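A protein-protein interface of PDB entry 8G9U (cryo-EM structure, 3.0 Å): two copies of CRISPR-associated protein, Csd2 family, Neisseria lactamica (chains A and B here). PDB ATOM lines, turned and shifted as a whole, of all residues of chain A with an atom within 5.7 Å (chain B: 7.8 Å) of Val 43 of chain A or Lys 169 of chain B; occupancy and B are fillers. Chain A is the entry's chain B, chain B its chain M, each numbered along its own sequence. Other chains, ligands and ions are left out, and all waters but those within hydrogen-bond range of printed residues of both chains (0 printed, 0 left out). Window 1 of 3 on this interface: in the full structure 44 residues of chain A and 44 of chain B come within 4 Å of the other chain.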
ATOM      1  N   ASN A  20      18.120  -3.731  32.523  1.00  0.00           N
ATOM      2  CA  ASN A  20      17.780  -2.938  31.357  1.00  0.00           C
ATOM      3  C   ASN A  20      16.992  -3.877  30.453  1.00  0.00           C
ATOM      4  O   ASN A  20      17.582  -4.715  29.772  1.00  0.00           O
ATOM      5  CB  ASN A  20      19.024  -2.410  30.680  1.00  0.00           C
ATOM      6  CG  ASN A  20      18.734  -1.787  29.364  1.00  0.00           C
ATOM      7  OD1 ASN A  20      18.538  -2.470  28.370  1.00  0.00           O
ATOM      8  ND2 ASN A  20      18.688  -0.473  29.340  1.00  0.00           N
ATOM      9  N   THR A  41      22.568  -1.519  28.603  1.00  0.00           N
ATOM     10  CA  THR A  41      23.127  -0.698  27.555  1.00  0.00           C
ATOM     11  C   THR A  41      23.994   0.411  28.134  1.00  0.00           C
ATOM     12  O   THR A  41      23.993   0.685  29.331  1.00  0.00           O
ATOM     13  CB  THR A  41      22.015  -0.087  26.723  1.00  0.00           C
ATOM     14  OG1 THR A  41      21.040   0.466  27.606  1.00  0.00           O
ATOM     15  CG2 THR A  41      21.355  -1.131  25.891  1.00  0.00           C
ATOM     16  N   ASP A  42      24.767   1.040  27.253  1.00  0.00           N
ATOM     17  CA  ASP A  42      25.444   2.265  27.635  1.00  0.00           C
ATOM     18  C   ASP A  42      24.437   3.233  28.195  1.00  0.00           C
ATOM     19  O   ASP A  42      24.610   3.788  29.282  1.00  0.00           O
ATOM     20  CB  ASP A  42      26.117   2.896  26.426  1.00  0.00           C
ATOM     21  CG  ASP A  42      27.256   2.086  25.933  1.00  0.00           C
ATOM     22  OD1 ASP A  42      27.852   1.401  26.764  1.00  0.00           O
ATOM     23  OD2 ASP A  42      27.575   2.137  24.737  1.00  0.00           O
ATOM     24  N   VAL A  43      23.343   3.404  27.460  1.00  0.00           N
ATOM     25  CA  VAL A  43      22.384   4.438  27.747  1.00  0.00           C
ATOM     26  C   VAL A  43      21.650   4.167  29.034  1.00  0.00           C
ATOM     27  O   VAL A  43      21.184   5.103  29.666  1.00  0.00           O
ATOM     28  CB  VAL A  43      21.437   4.554  26.554  1.00  0.00           C
ATOM     29  CG1 VAL A  43      22.240   4.886  25.350  1.00  0.00           C
ATOM     30  CG2 VAL A  43      20.737   3.277  26.330  1.00  0.00           C
ATOM     31  N   CYS A  44      21.564   2.916  29.475  1.00  0.00           N
ATOM     32  CA  CYS A  44      20.896   2.650  30.741  1.00  0.00           C
ATOM     33  C   CYS A  44      21.679   3.224  31.907  1.00  0.00           C
ATOM     34  O   CYS A  44      21.131   3.945  32.741  1.00  0.00           O
ATOM     35  CB  CYS A  44      20.694   1.159  30.933  1.00  0.00           C
ATOM     36  SG  CYS A  44      19.712   0.765  32.378  1.00  0.00           S
ATOM     37  N   LEU A  45      22.968   2.918  31.986  1.00  0.00           N
ATOM     38  CA  LEU A  45      23.753   3.451  33.087  1.00  0.00           C
ATOM     39  C   LEU A  45      24.031   4.926  32.899  1.00  0.00           C
ATOM     40  O   LEU A  45      24.151   5.665  33.877  1.00  0.00           O
ATOM     41  CB  LEU A  45      25.048   2.685  33.225  1.00  0.00           C
ATOM     42  CG  LEU A  45      24.817   1.196  33.147  1.00  0.00           C
ATOM     43  CD1 LEU A  45      26.133   0.488  33.022  1.00  0.00           C
ATOM     44  CD2 LEU A  45      24.093   0.790  34.386  1.00  0.00           C
ATOM     45  N   LYS A  46      24.124   5.376  31.659  1.00  0.00           N
ATOM     46  CA  LYS A  46      24.214   6.806  31.438  1.00  0.00           C
ATOM     47  C   LYS A  46      22.954   7.501  31.923  1.00  0.00           C
ATOM     48  O   LYS A  46      23.027   8.570  32.524  1.00  0.00           O
ATOM     49  CB  LYS A  46      24.484   7.081  29.964  1.00  0.00           C
ATOM     50  CG  LYS A  46      25.847   6.604  29.509  1.00  0.00           C
ATOM     51  CD  LYS A  46      26.005   6.766  28.029  1.00  0.00           C
ATOM     52  CE  LYS A  46      27.417   6.516  27.591  1.00  0.00           C
ATOM     53  NZ  LYS A  46      27.803   7.419  26.480  1.00  0.00           N
ATOM     54  N   ARG A  47      21.792   6.886  31.725  1.00  0.00           N
ATOM     55  CA  ARG A  47      20.544   7.461  32.204  1.00  0.00           C
ATOM     56  C   ARG A  47      20.456   7.394  33.709  1.00  0.00           C
ATOM     57  O   ARG A  47      19.829   8.240  34.338  1.00  0.00           O
ATOM     58  CB  ARG A  47      19.365   6.712  31.622  1.00  0.00           C
ATOM     59  CG  ARG A  47      18.016   7.173  32.126  1.00  0.00           C
ATOM     60  CD  ARG A  47      17.553   8.432  31.451  1.00  0.00           C
ATOM     61  NE  ARG A  47      17.867   9.668  32.136  1.00  0.00           N
ATOM     62  CZ  ARG A  47      17.631  10.857  31.606  1.00  0.00           C
ATOM     63  NH1 ARG A  47      17.106  10.937  30.401  1.00  0.00           N
ATOM     64  NH2 ARG A  47      17.921  11.961  32.268  1.00  0.00           N
ATOM     65  N   LYS A  48      21.020   6.359  34.306  1.00  0.00           N
ATOM     66  CA  LYS A  48      20.963   6.290  35.754  1.00  0.00           C
ATOM     67  C   LYS A  48      21.899   7.310  36.381  1.00  0.00           C
ATOM     68  O   LYS A  48      21.566   7.904  37.412  1.00  0.00           O
ATOM     69  CB  LYS A  48      21.243   4.867  36.206  1.00  0.00           C
ATOM     70  CG  LYS A  48      20.097   3.963  35.841  1.00  0.00           C
ATOM     71  CD  LYS A  48      20.428   2.516  35.974  1.00  0.00           C
ATOM     72  CE  LYS A  48      19.191   1.674  35.771  1.00  0.00           C
ATOM     73  NZ  LYS A  48      18.538   1.951  34.470  1.00  0.00           N
ATOM     74  N   ARG A  50      22.358  10.123  34.805  1.00  0.00           N
ATOM     75  CA  ARG A  50      21.542  11.298  34.538  1.00  0.00           C
ATOM     76  C   ARG A  50      20.498  11.497  35.615  1.00  0.00           C
ATOM     77  O   ARG A  50      20.246  12.621  36.046  1.00  0.00           O
ATOM     78  CB  ARG A  50      20.846  11.148  33.201  1.00  0.00           C
ATOM     79  CG  ARG A  50      21.720  11.261  32.028  1.00  0.00           C
ATOM     80  CD  ARG A  50      20.880  11.166  30.811  1.00  0.00           C
ATOM     81  NE  ARG A  50      21.699  11.380  29.648  1.00  0.00           N
ATOM     82  CZ  ARG A  50      22.258  10.413  28.947  1.00  0.00           C
ATOM     83  NH1 ARG A  50      22.078   9.147  29.273  1.00  0.00           N
ATOM     84  NH2 ARG A  50      23.015  10.747  27.926  1.00  0.00           N
ATOM     85  N   PHE A 132      28.576  -1.341  27.143  1.00  0.00           N
ATOM     86  CA  PHE A 132      27.473  -2.229  27.463  1.00  0.00           C
ATOM     87  C   PHE A 132      27.925  -3.214  28.518  1.00  0.00           C
ATOM     88  O   PHE A 132      28.782  -4.061  28.261  1.00  0.00           O
ATOM     89  CB  PHE A 132      26.988  -2.964  26.226  1.00  0.00           C
ATOM     90  CG  PHE A 132      26.177  -2.123  25.325  1.00  0.00           C
ATOM     91  CD1 PHE A 132      26.716  -0.999  24.744  1.00  0.00           C
ATOM     92  CD2 PHE A 132      24.867  -2.430  25.078  1.00  0.00           C
ATOM     93  CE1 PHE A 132      25.965  -0.212  23.918  1.00  0.00           C
ATOM     94  CE2 PHE A 132      24.120  -1.643  24.252  1.00  0.00           C
ATOM     95  CZ  PHE A 132      24.664  -0.531  23.678  1.00  0.00           C
ATOM     96  N   ASP B  16      31.886  -4.603  23.480  1.00  0.00           N
ATOM     97  CA  ASP B  16      30.453  -4.461  23.668  1.00  0.00           C
ATOM     98  C   ASP B  16      29.902  -3.338  22.822  1.00  0.00           C
ATOM     99  O   ASP B  16      29.021  -2.593  23.253  1.00  0.00           O
ATOM    100  CB  ASP B  16      30.125  -4.232  25.133  1.00  0.00           C
ATOM    101  CG  ASP B  16      29.893  -5.513  25.870  1.00  0.00           C
ATOM    102  OD1 ASP B  16      29.045  -6.308  25.416  1.00  0.00           O
ATOM    103  OD2 ASP B  16      30.573  -5.727  26.894  1.00  0.00           O
ATOM    104  N   GLY B  17      30.399  -3.187  21.610  1.00  0.00           N
ATOM    105  CA  GLY B  17      30.017  -2.003  20.886  1.00  0.00           C
ATOM    106  C   GLY B  17      29.849  -2.162  19.400  1.00  0.00           C
ATOM    107  O   GLY B  17      29.864  -3.268  18.860  1.00  0.00           O
ATOM    108  N   ASN B  18      29.673  -1.035  18.737  1.00  0.00           N
ATOM    109  CA  ASN B  18      29.508  -0.978  17.300  1.00  0.00           C
ATOM    110  C   ASN B  18      30.834  -0.552  16.713  1.00  0.00           C
ATOM    111  O   ASN B  18      31.151   0.644  16.725  1.00  0.00           O
ATOM    112  CB  ASN B  18      28.406   0.014  16.935  1.00  0.00           C
ATOM    113  CG  ASN B  18      28.305   0.250  15.464  1.00  0.00           C
ATOM    114  OD1 ASN B  18      29.108   0.968  14.879  1.00  0.00           O
ATOM    115  ND2 ASN B  18      27.311  -0.354  14.847  1.00  0.00           N
ATOM    116  N   ASN B  27      22.779   1.803  11.799  1.00  0.00           N
ATOM    117  CA  ASN B  27      24.114   1.880  12.365  1.00  0.00           C
ATOM    118  C   ASN B  27      24.636   0.515  12.775  1.00  0.00           C
ATOM    119  O   ASN B  27      25.587   0.448  13.555  1.00  0.00           O
ATOM    120  CB  ASN B  27      24.117   2.824  13.559  1.00  0.00           C
ATOM    121  CG  ASN B  27      25.470   3.409  13.828  1.00  0.00           C
ATOM    122  OD1 ASN B  27      26.469   2.916  13.334  1.00  0.00           O
ATOM    123  ND2 ASN B  27      25.513   4.475  14.616  1.00  0.00           N
ATOM    124  N   LEU B  28      24.037  -0.571  12.309  1.00  0.00           N
ATOM    125  CA  LEU B  28      24.458  -1.873  12.786  1.00  0.00           C
ATOM    126  C   LEU B  28      25.846  -2.190  12.254  1.00  0.00           C
ATOM    127  O   LEU B  28      26.181  -1.805  11.133  1.00  0.00           O
ATOM    128  CB  LEU B  28      23.464  -2.959  12.389  1.00  0.00           C
ATOM    129  CG  LEU B  28      23.138  -3.329  10.953  1.00  0.00           C
ATOM    130  CD1 LEU B  28      24.043  -4.438  10.453  1.00  0.00           C
ATOM    131  CD2 LEU B  28      21.700  -3.779  10.920  1.00  0.00           C
ATOM    132  N   PRO B  29      26.676  -2.864  13.042  1.00  0.00           N
ATOM    133  CA  PRO B  29      28.059  -3.077  12.636  1.00  0.00           C
ATOM    134  C   PRO B  29      28.111  -3.773  11.296  1.00  0.00           C
ATOM    135  O   PRO B  29      27.322  -4.676  11.020  1.00  0.00           O
ATOM    136  CB  PRO B  29      28.618  -3.959  13.753  1.00  0.00           C
ATOM    137  CG  PRO B  29      27.735  -3.707  14.895  1.00  0.00           C
ATOM    138  CD  PRO B  29      26.390  -3.483  14.337  1.00  0.00           C
ATOM    139  N   THR B 141      25.810  -9.204  15.772  1.00  0.00           N
ATOM    140  CA  THR B 141      25.261  -7.877  15.990  1.00  0.00           C
ATOM    141  C   THR B 141      24.007  -7.958  16.842  1.00  0.00           C
ATOM    142  O   THR B 141      23.023  -8.593  16.455  1.00  0.00           O
ATOM    143  CB  THR B 141      24.950  -7.209  14.659  1.00  0.00           C
ATOM    144  OG1 THR B 141      26.169  -6.774  14.052  1.00  0.00           O
ATOM    145  CG2 THR B 141      24.037  -6.027  14.865  1.00  0.00           C
ATOM    146  N   LEU B 142      24.042  -7.348  18.015  1.00  0.00           N
ATOM    147  CA  LEU B 142      22.911  -7.379  18.931  1.00  0.00           C
ATOM    148  C   LEU B 142      22.138  -6.087  18.752  1.00  0.00           C
ATOM    149  O   LEU B 142      22.560  -5.031  19.217  1.00  0.00           O
ATOM    150  CB  LEU B 142      23.389  -7.549  20.363  1.00  0.00           C
ATOM    151  CG  LEU B 142      23.978  -8.916  20.655  1.00  0.00           C
ATOM    152  CD1 LEU B 142      24.042  -9.141  22.131  1.00  0.00           C
ATOM    153  CD2 LEU B 142      23.148  -9.980  19.990  1.00  0.00           C
ATOM    154  N   GLU B 143      21.002  -6.166  18.082  1.00  0.00           N
ATOM    155  CA  GLU B 143      20.182  -4.985  17.856  1.00  0.00           C
ATOM    156  C   GLU B 143      19.548  -4.597  19.180  1.00  0.00           C
ATOM    157  O   GLU B 143      18.495  -5.109  19.553  1.00  0.00           O
ATOM    158  CB  GLU B 143      19.121  -5.274  16.804  1.00  0.00           C
ATOM    159  CG  GLU B 143      19.677  -5.661  15.450  1.00  0.00           C
ATOM    160  CD  GLU B 143      19.847  -7.154  15.303  1.00  0.00           C
ATOM    161  OE1 GLU B 143      19.443  -7.891  16.225  1.00  0.00           O
ATOM    162  OE2 GLU B 143      20.384  -7.593  14.266  1.00  0.00           O
ATOM    163  N   HIS B 144      20.193  -3.702  19.910  1.00  0.00           N
ATOM    164  CA  HIS B 144      19.684  -3.232  21.188  1.00  0.00           C
ATOM    165  C   HIS B 144      18.826  -2.009  20.935  1.00  0.00           C
ATOM    166  O   HIS B 144      19.348  -0.908  20.754  1.00  0.00           O
ATOM    167  CB  HIS B 144      20.817  -2.894  22.144  1.00  0.00           C
ATOM    168  CG  HIS B 144      21.645  -4.067  22.528  1.00  0.00           C
ATOM    169  ND1 HIS B 144      22.996  -3.976  22.757  1.00  0.00           N
ATOM    170  CD2 HIS B 144      21.311  -5.360  22.733  1.00  0.00           C
ATOM    171  CE1 HIS B 144      23.461  -5.164  23.092  1.00  0.00           C
ATOM    172  NE2 HIS B 144      22.460  -6.022  23.079  1.00  0.00           N
ATOM    173  N   SER B 145      17.518  -2.195  20.922  1.00  0.00           N
ATOM    174  CA  SER B 145      16.615  -1.070  20.770  1.00  0.00           C
ATOM    175  C   SER B 145      16.640  -0.287  22.062  1.00  0.00           C
ATOM    176  O   SER B 145      16.089  -0.728  23.071  1.00  0.00           O
ATOM    177  CB  SER B 145      15.208  -1.536  20.452  1.00  0.00           C
ATOM    178  OG  SER B 145      15.090  -1.957  19.107  1.00  0.00           O
ATOM    179  N   ILE B 146      17.290   0.864  22.041  1.00  0.00           N
ATOM    180  CA  ILE B 146      17.386   1.697  23.197  1.00  0.00           C
ATOM    181  C   ILE B 146      16.277   2.734  23.146  1.00  0.00           C
ATOM    182  O   ILE B 146      15.673   2.983  22.108  1.00  0.00           O
ATOM    183  CB  ILE B 146      18.757   2.359  23.309  1.00  0.00           C
ATOM    184  CG1 ILE B 146      18.941   3.327  22.168  1.00  0.00           C
ATOM    185  CG2 ILE B 146      19.842   1.329  23.284  1.00  0.00           C
ATOM    186  CD1 ILE B 146      20.232   3.983  22.231  1.00  0.00           C
ATOM    187  N   THR B 147      16.001   3.340  24.283  1.00  0.00           N
ATOM    188  CA  THR B 147      14.954   4.328  24.422  1.00  0.00           C
ATOM    189  C   THR B 147      15.605   5.635  24.830  1.00  0.00           C
ATOM    190  O   THR B 147      16.664   5.636  25.453  1.00  0.00           O
ATOM    191  CB  THR B 147      13.949   3.872  25.469  1.00  0.00           C
ATOM    192  OG1 THR B 147      13.383   2.627  25.057  1.00  0.00           O
ATOM    193  CG2 THR B 147      12.825   4.867  25.627  1.00  0.00           C
ATOM    194  N   ARG B 148      15.002   6.751  24.453  1.00  0.00           N
ATOM    195  CA  ARG B 148      15.383   8.027  25.031  1.00  0.00           C
ATOM    196  C   ARG B 148      14.177   8.629  25.719  1.00  0.00           C
ATOM    197  O   ARG B 148      13.074   8.633  25.171  1.00  0.00           O
ATOM    198  CB  ARG B 148      15.919   9.007  24.009  1.00  0.00           C
ATOM    199  CG  ARG B 148      16.352  10.299  24.658  1.00  0.00           C
ATOM    200  CD  ARG B 148      17.209  11.119  23.756  1.00  0.00           C
ATOM    201  NE  ARG B 148      16.584  11.239  22.461  1.00  0.00           N
ATOM    202  CZ  ARG B 148      17.180  11.732  21.391  1.00  0.00           C
ATOM    203  NH1 ARG B 148      18.427  12.161  21.469  1.00  0.00           N
ATOM    204  NH2 ARG B 148      16.530  11.794  20.245  1.00  0.00           N
ATOM    205  N   MET B 149      14.389   9.135  26.922  1.00  0.00           N
ATOM    206  CA  MET B 149      13.287   9.685  27.689  1.00  0.00           C
ATOM    207  C   MET B 149      13.026  11.119  27.295  1.00  0.00           C
ATOM    208  O   MET B 149      12.823  11.980  28.151  1.00  0.00           O
ATOM    209  CB  MET B 149      13.641   9.581  29.162  1.00  0.00           C
ATOM    210  CG  MET B 149      13.734   8.150  29.599  1.00  0.00           C
ATOM    211  SD  MET B 149      14.222   7.949  31.302  1.00  0.00           S
ATOM    212  CE  MET B 149      12.758   8.505  32.109  1.00  0.00           C
ATOM    213  N   GLY B 167      14.778   4.189  20.269  1.00  0.00           N
ATOM    214  CA  GLY B 167      15.875   4.268  19.332  1.00  0.00           C
ATOM    215  C   GLY B 167      16.471   2.930  18.982  1.00  0.00           C
ATOM    216  O   GLY B 167      15.778   1.912  18.985  1.00  0.00           O
ATOM    217  N   ARG B 168      17.754   2.922  18.650  1.00  0.00           N
ATOM    218  CA  ARG B 168      18.417   1.697  18.232  1.00  0.00           C
ATOM    219  C   ARG B 168      19.915   1.863  18.386  1.00  0.00           C
ATOM    220  O   ARG B 168      20.497   2.785  17.811  1.00  0.00           O
ATOM    221  CB  ARG B 168      18.069   1.367  16.792  1.00  0.00           C
ATOM    222  CG  ARG B 168      18.684   0.099  16.340  1.00  0.00           C
ATOM    223  CD  ARG B 168      18.116  -1.046  17.106  1.00  0.00           C
ATOM    224  NE  ARG B 168      16.684  -1.111  16.898  1.00  0.00           N
ATOM    225  CZ  ARG B 168      16.126  -1.712  15.862  1.00  0.00           C
ATOM    226  NH1 ARG B 168      14.809  -1.720  15.736  1.00  0.00           N
ATOM    227  NH2 ARG B 168      16.886  -2.311  14.959  1.00  0.00           N
ATOM    228  N   LYS B 169      20.537   0.968  19.139  1.00  0.00           N
ATOM    229  CA  LYS B 169      21.978   0.980  19.322  1.00  0.00           C
ATOM    230  C   LYS B 169      22.478  -0.446  19.272  1.00  0.00           C
ATOM    231  O   LYS B 169      22.068  -1.273  20.084  1.00  0.00           O
ATOM    232  CB  LYS B 169      22.370   1.626  20.646  1.00  0.00           C
ATOM    233  CG  LYS B 169      23.850   1.694  20.869  1.00  0.00           C
ATOM    234  CD  LYS B 169      24.167   2.448  22.129  1.00  0.00           C
ATOM    235  CE  LYS B 169      23.980   3.924  21.892  1.00  0.00           C
ATOM    236  NZ  LYS B 169      24.434   4.728  23.042  1.00  0.00           N
ATOM    237  N   PHE B 170      23.366  -0.725  18.337  1.00  0.00           N
ATOM    238  CA  PHE B 170      23.826  -2.079  18.101  1.00  0.00           C
ATOM    239  C   PHE B 170      25.132  -2.323  18.825  1.00  0.00           C
ATOM    240  O   PHE B 170      25.892  -1.395  19.103  1.00  0.00           O
ATOM    241  CB  PHE B 170      24.029  -2.332  16.622  1.00  0.00           C
ATOM    242  CG  PHE B 170      22.863  -1.972  15.791  1.00  0.00           C
ATOM    243  CD1 PHE B 170      22.688  -0.683  15.354  1.00  0.00           C
ATOM    244  CD2 PHE B 170      21.944  -2.923  15.436  1.00  0.00           C
ATOM    245  CE1 PHE B 170      21.626  -0.355  14.577  1.00  0.00           C
ATOM    246  CE2 PHE B 170      20.879  -2.598  14.658  1.00  0.00           C
ATOM    247  CZ  PHE B 170      20.722  -1.318  14.223  1.00  0.00           C
ATOM    248  N   THR B 171      25.386  -3.586  19.133  1.00  0.00           N
ATOM    249  CA  THR B 171      26.659  -3.981  19.694  1.00  0.00           C
ATOM    250  C   THR B 171      27.131  -5.238  19.004  1.00  0.00           C
ATOM    251  O   THR B 171      26.334  -6.031  18.504  1.00  0.00           O
ATOM    252  CB  THR B 171      26.596  -4.286  21.180  1.00  0.00           C
ATOM    253  OG1 THR B 171      25.705  -5.380  21.394  1.00  0.00           O
ATOM    254  CG2 THR B 171      26.095  -3.103  21.924  1.00  0.00           C
ATOM    255  N   VAL B 172      28.445  -5.412  18.991  1.00  0.00           N
ATOM    256  CA  VAL B 172      29.057  -6.708  18.744  1.00  0.00           C
ATOM    257  C   VAL B 172      29.461  -7.265  20.103  1.00  0.00           C
ATOM    258  O   VAL B 172      30.335  -6.682  20.760  1.00  0.00           O
ATOM    259  CB  VAL B 172      30.262  -6.582  17.814  1.00  0.00           C
ATOM    260  CG1 VAL B 172      30.922  -7.911  17.664  1.00  0.00           C
ATOM    261  CG2 VAL B 172      29.826  -6.056  16.493  1.00  0.00           C
ATOM    262  N   SER B 214      33.338   5.828  22.868  1.00  0.00           N
ATOM    263  CA  SER B 214      32.069   6.456  22.553  1.00  0.00           C
ATOM    264  C   SER B 214      30.950   5.631  23.154  1.00  0.00           C
ATOM    265  O   SER B 214      31.182   4.659  23.876  1.00  0.00           O
ATOM    266  CB  SER B 214      31.895   6.585  21.051  1.00  0.00           C
ATOM    267  OG  SER B 214      30.532   6.771  20.750  1.00  0.00           O
ATOM    268  N   ALA B 215      29.723   6.031  22.853  1.00  0.00           N
ATOM    269  CA  ALA B 215      28.594   5.188  23.204  1.00  0.00           C
ATOM    270  C   ALA B 215      28.383   4.117  22.148  1.00  0.00           C
ATOM    271  O   ALA B 215      28.269   2.932  22.467  1.00  0.00           O
ATOM    272  CB  ALA B 215      27.339   6.034  23.374  1.00  0.00           C
ATOM    273  N   ALA B 216      28.354   4.508  20.881  1.00  0.00           N
ATOM    274  CA  ALA B 216      28.177   3.517  19.832  1.00  0.00           C
ATOM    275  C   ALA B 216      29.313   2.508  19.847  1.00  0.00           C
ATOM    276  O   ALA B 216      29.085   1.301  19.728  1.00  0.00           O
ATOM    277  CB  ALA B 216      28.080   4.201  18.472  1.00  0.00           C
ATOM    278  N   ARG B 217      30.543   2.976  20.026  1.00  0.00           N
ATOM    279  CA  ARG B 217      31.689   2.101  19.826  1.00  0.00           C
ATOM    280  C   ARG B 217      32.053   1.279  21.044  1.00  0.00           C
ATOM    281  O   ARG B 217      32.996   0.492  20.962  1.00  0.00           O
ATOM    282  CB  ARG B 217      32.897   2.903  19.356  1.00  0.00           C
ATOM    283  CG  ARG B 217      32.938   2.974  17.853  1.00  0.00           C
ATOM    284  CD  ARG B 217      34.162   3.636  17.340  1.00  0.00           C
ATOM    285  NE  ARG B 217      33.971   5.070  17.235  1.00  0.00           N
ATOM    286  CZ  ARG B 217      34.786   5.963  17.770  1.00  0.00           C
ATOM    287  NH1 ARG B 217      35.836   5.554  18.457  1.00  0.00           N
ATOM    288  NH2 ARG B 217      34.546   7.257  17.623  1.00  0.00           N
ATOM    289  N   GLY B 218      31.336   1.430  22.149  1.00  0.00           N
ATOM    290  CA  GLY B 218      31.542   0.542  23.280  1.00  0.00           C
ATOM    291  C   GLY B 218      32.995   0.502  23.690  1.00  0.00           C
ATOM    292  O   GLY B 218      33.692   1.520  23.696  1.00  0.00           O
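The side-chain carboxylate (OD2) of Asp 42 of chain A lies close to the backbone carbonyl oxygen (O) of Ala 215 of chain B, at 2.5 Å. O of Phe 132 of chain A sits close to OD2 of Asp 16 of chain B, at 2.8 Å.
No position is printed for both chains. Of the 10 pairs that touch across the chains among the printed residues, none has its exchanged pair printed and touching as well.
The side-chain hydroxyl (OG1) of Thr 41 of chain A sits at hydrogen-bond distance from the side-chain amide nitrogen (ND2) of Asn 20 of chain A (3.1 Å). The side-chain hydroxyl of Thr 41 of chain A lies within hydrogen-bond range of the backbone NH of Cys 44 of chain A (3.1 Å). The side-chain carboxylate of Asp 42 of chain A lies within hydrogen-bond range of the backbone NH of Phe 132 of chain A, 2.9 Å away. NH1 of Arg 50 of chain A lies close to O of Lys 46 of chain A (3.4 Å). The backbone NH (N) of Leu 142 of chain B sits at hydrogen-bond distance from the backbone carbonyl oxygen (O) of Thr 171 of chain B (2.7 Å). O of His 144 of chain B sits at hydrogen-bond distance from N of Lys 169 of chain B, at 2.7 Å.
Of the 26 printed residues of chain B, 7 touch a printed residue of chain A. Among the printed residues, 10 pairs touch across the chains. Among the printed residues, no Asp or Glu carboxylate lies within 4 Å of a Lys or Arg side-chain nitrogen of the other chain.
Thr 41 of chain A touches Ile 146 of chain B (CG2 to CG2, 3.9 Å). Ile 146 of chain B touches Val 43 of chain A (CG2 to CG2, 3.7 Å). Val 43 of chain A touches Lys 169 of chain B (CG1 to NZ, 3.2 Å). NZ of Lys 46 of chain A touches CB of Ala 215 of chain B (3.4 Å). Met 149 of chain B touches Arg 47 of chain A (SD to CD, 3.4 Å). His 144 of chain B touches Phe 132 of chain A. Lys 169 of chain B touches Phe 132 of chain A. Phe 132 of chain A touches Thr 171 of chain B.
Of chain B, only Ile 146 and Lys 169 come within 4 Å of Val 43 of chain A. Of the printed residues of chain B, Lys 46 of chain A touches Ala 215. Of the printed residues of chain A, Asp 16 of chain B touches Phe 132. Printed residues of chain A within 4 Å of Met 149 of chain B: Arg 47 (3.4 Å). Of chain A, only Val 43 and Phe 132 come within 4 Å of Lys 169 of chain B. Of the printed residues of chain A, Thr 171 of chain B touches Phe 132 (3.4 Å).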
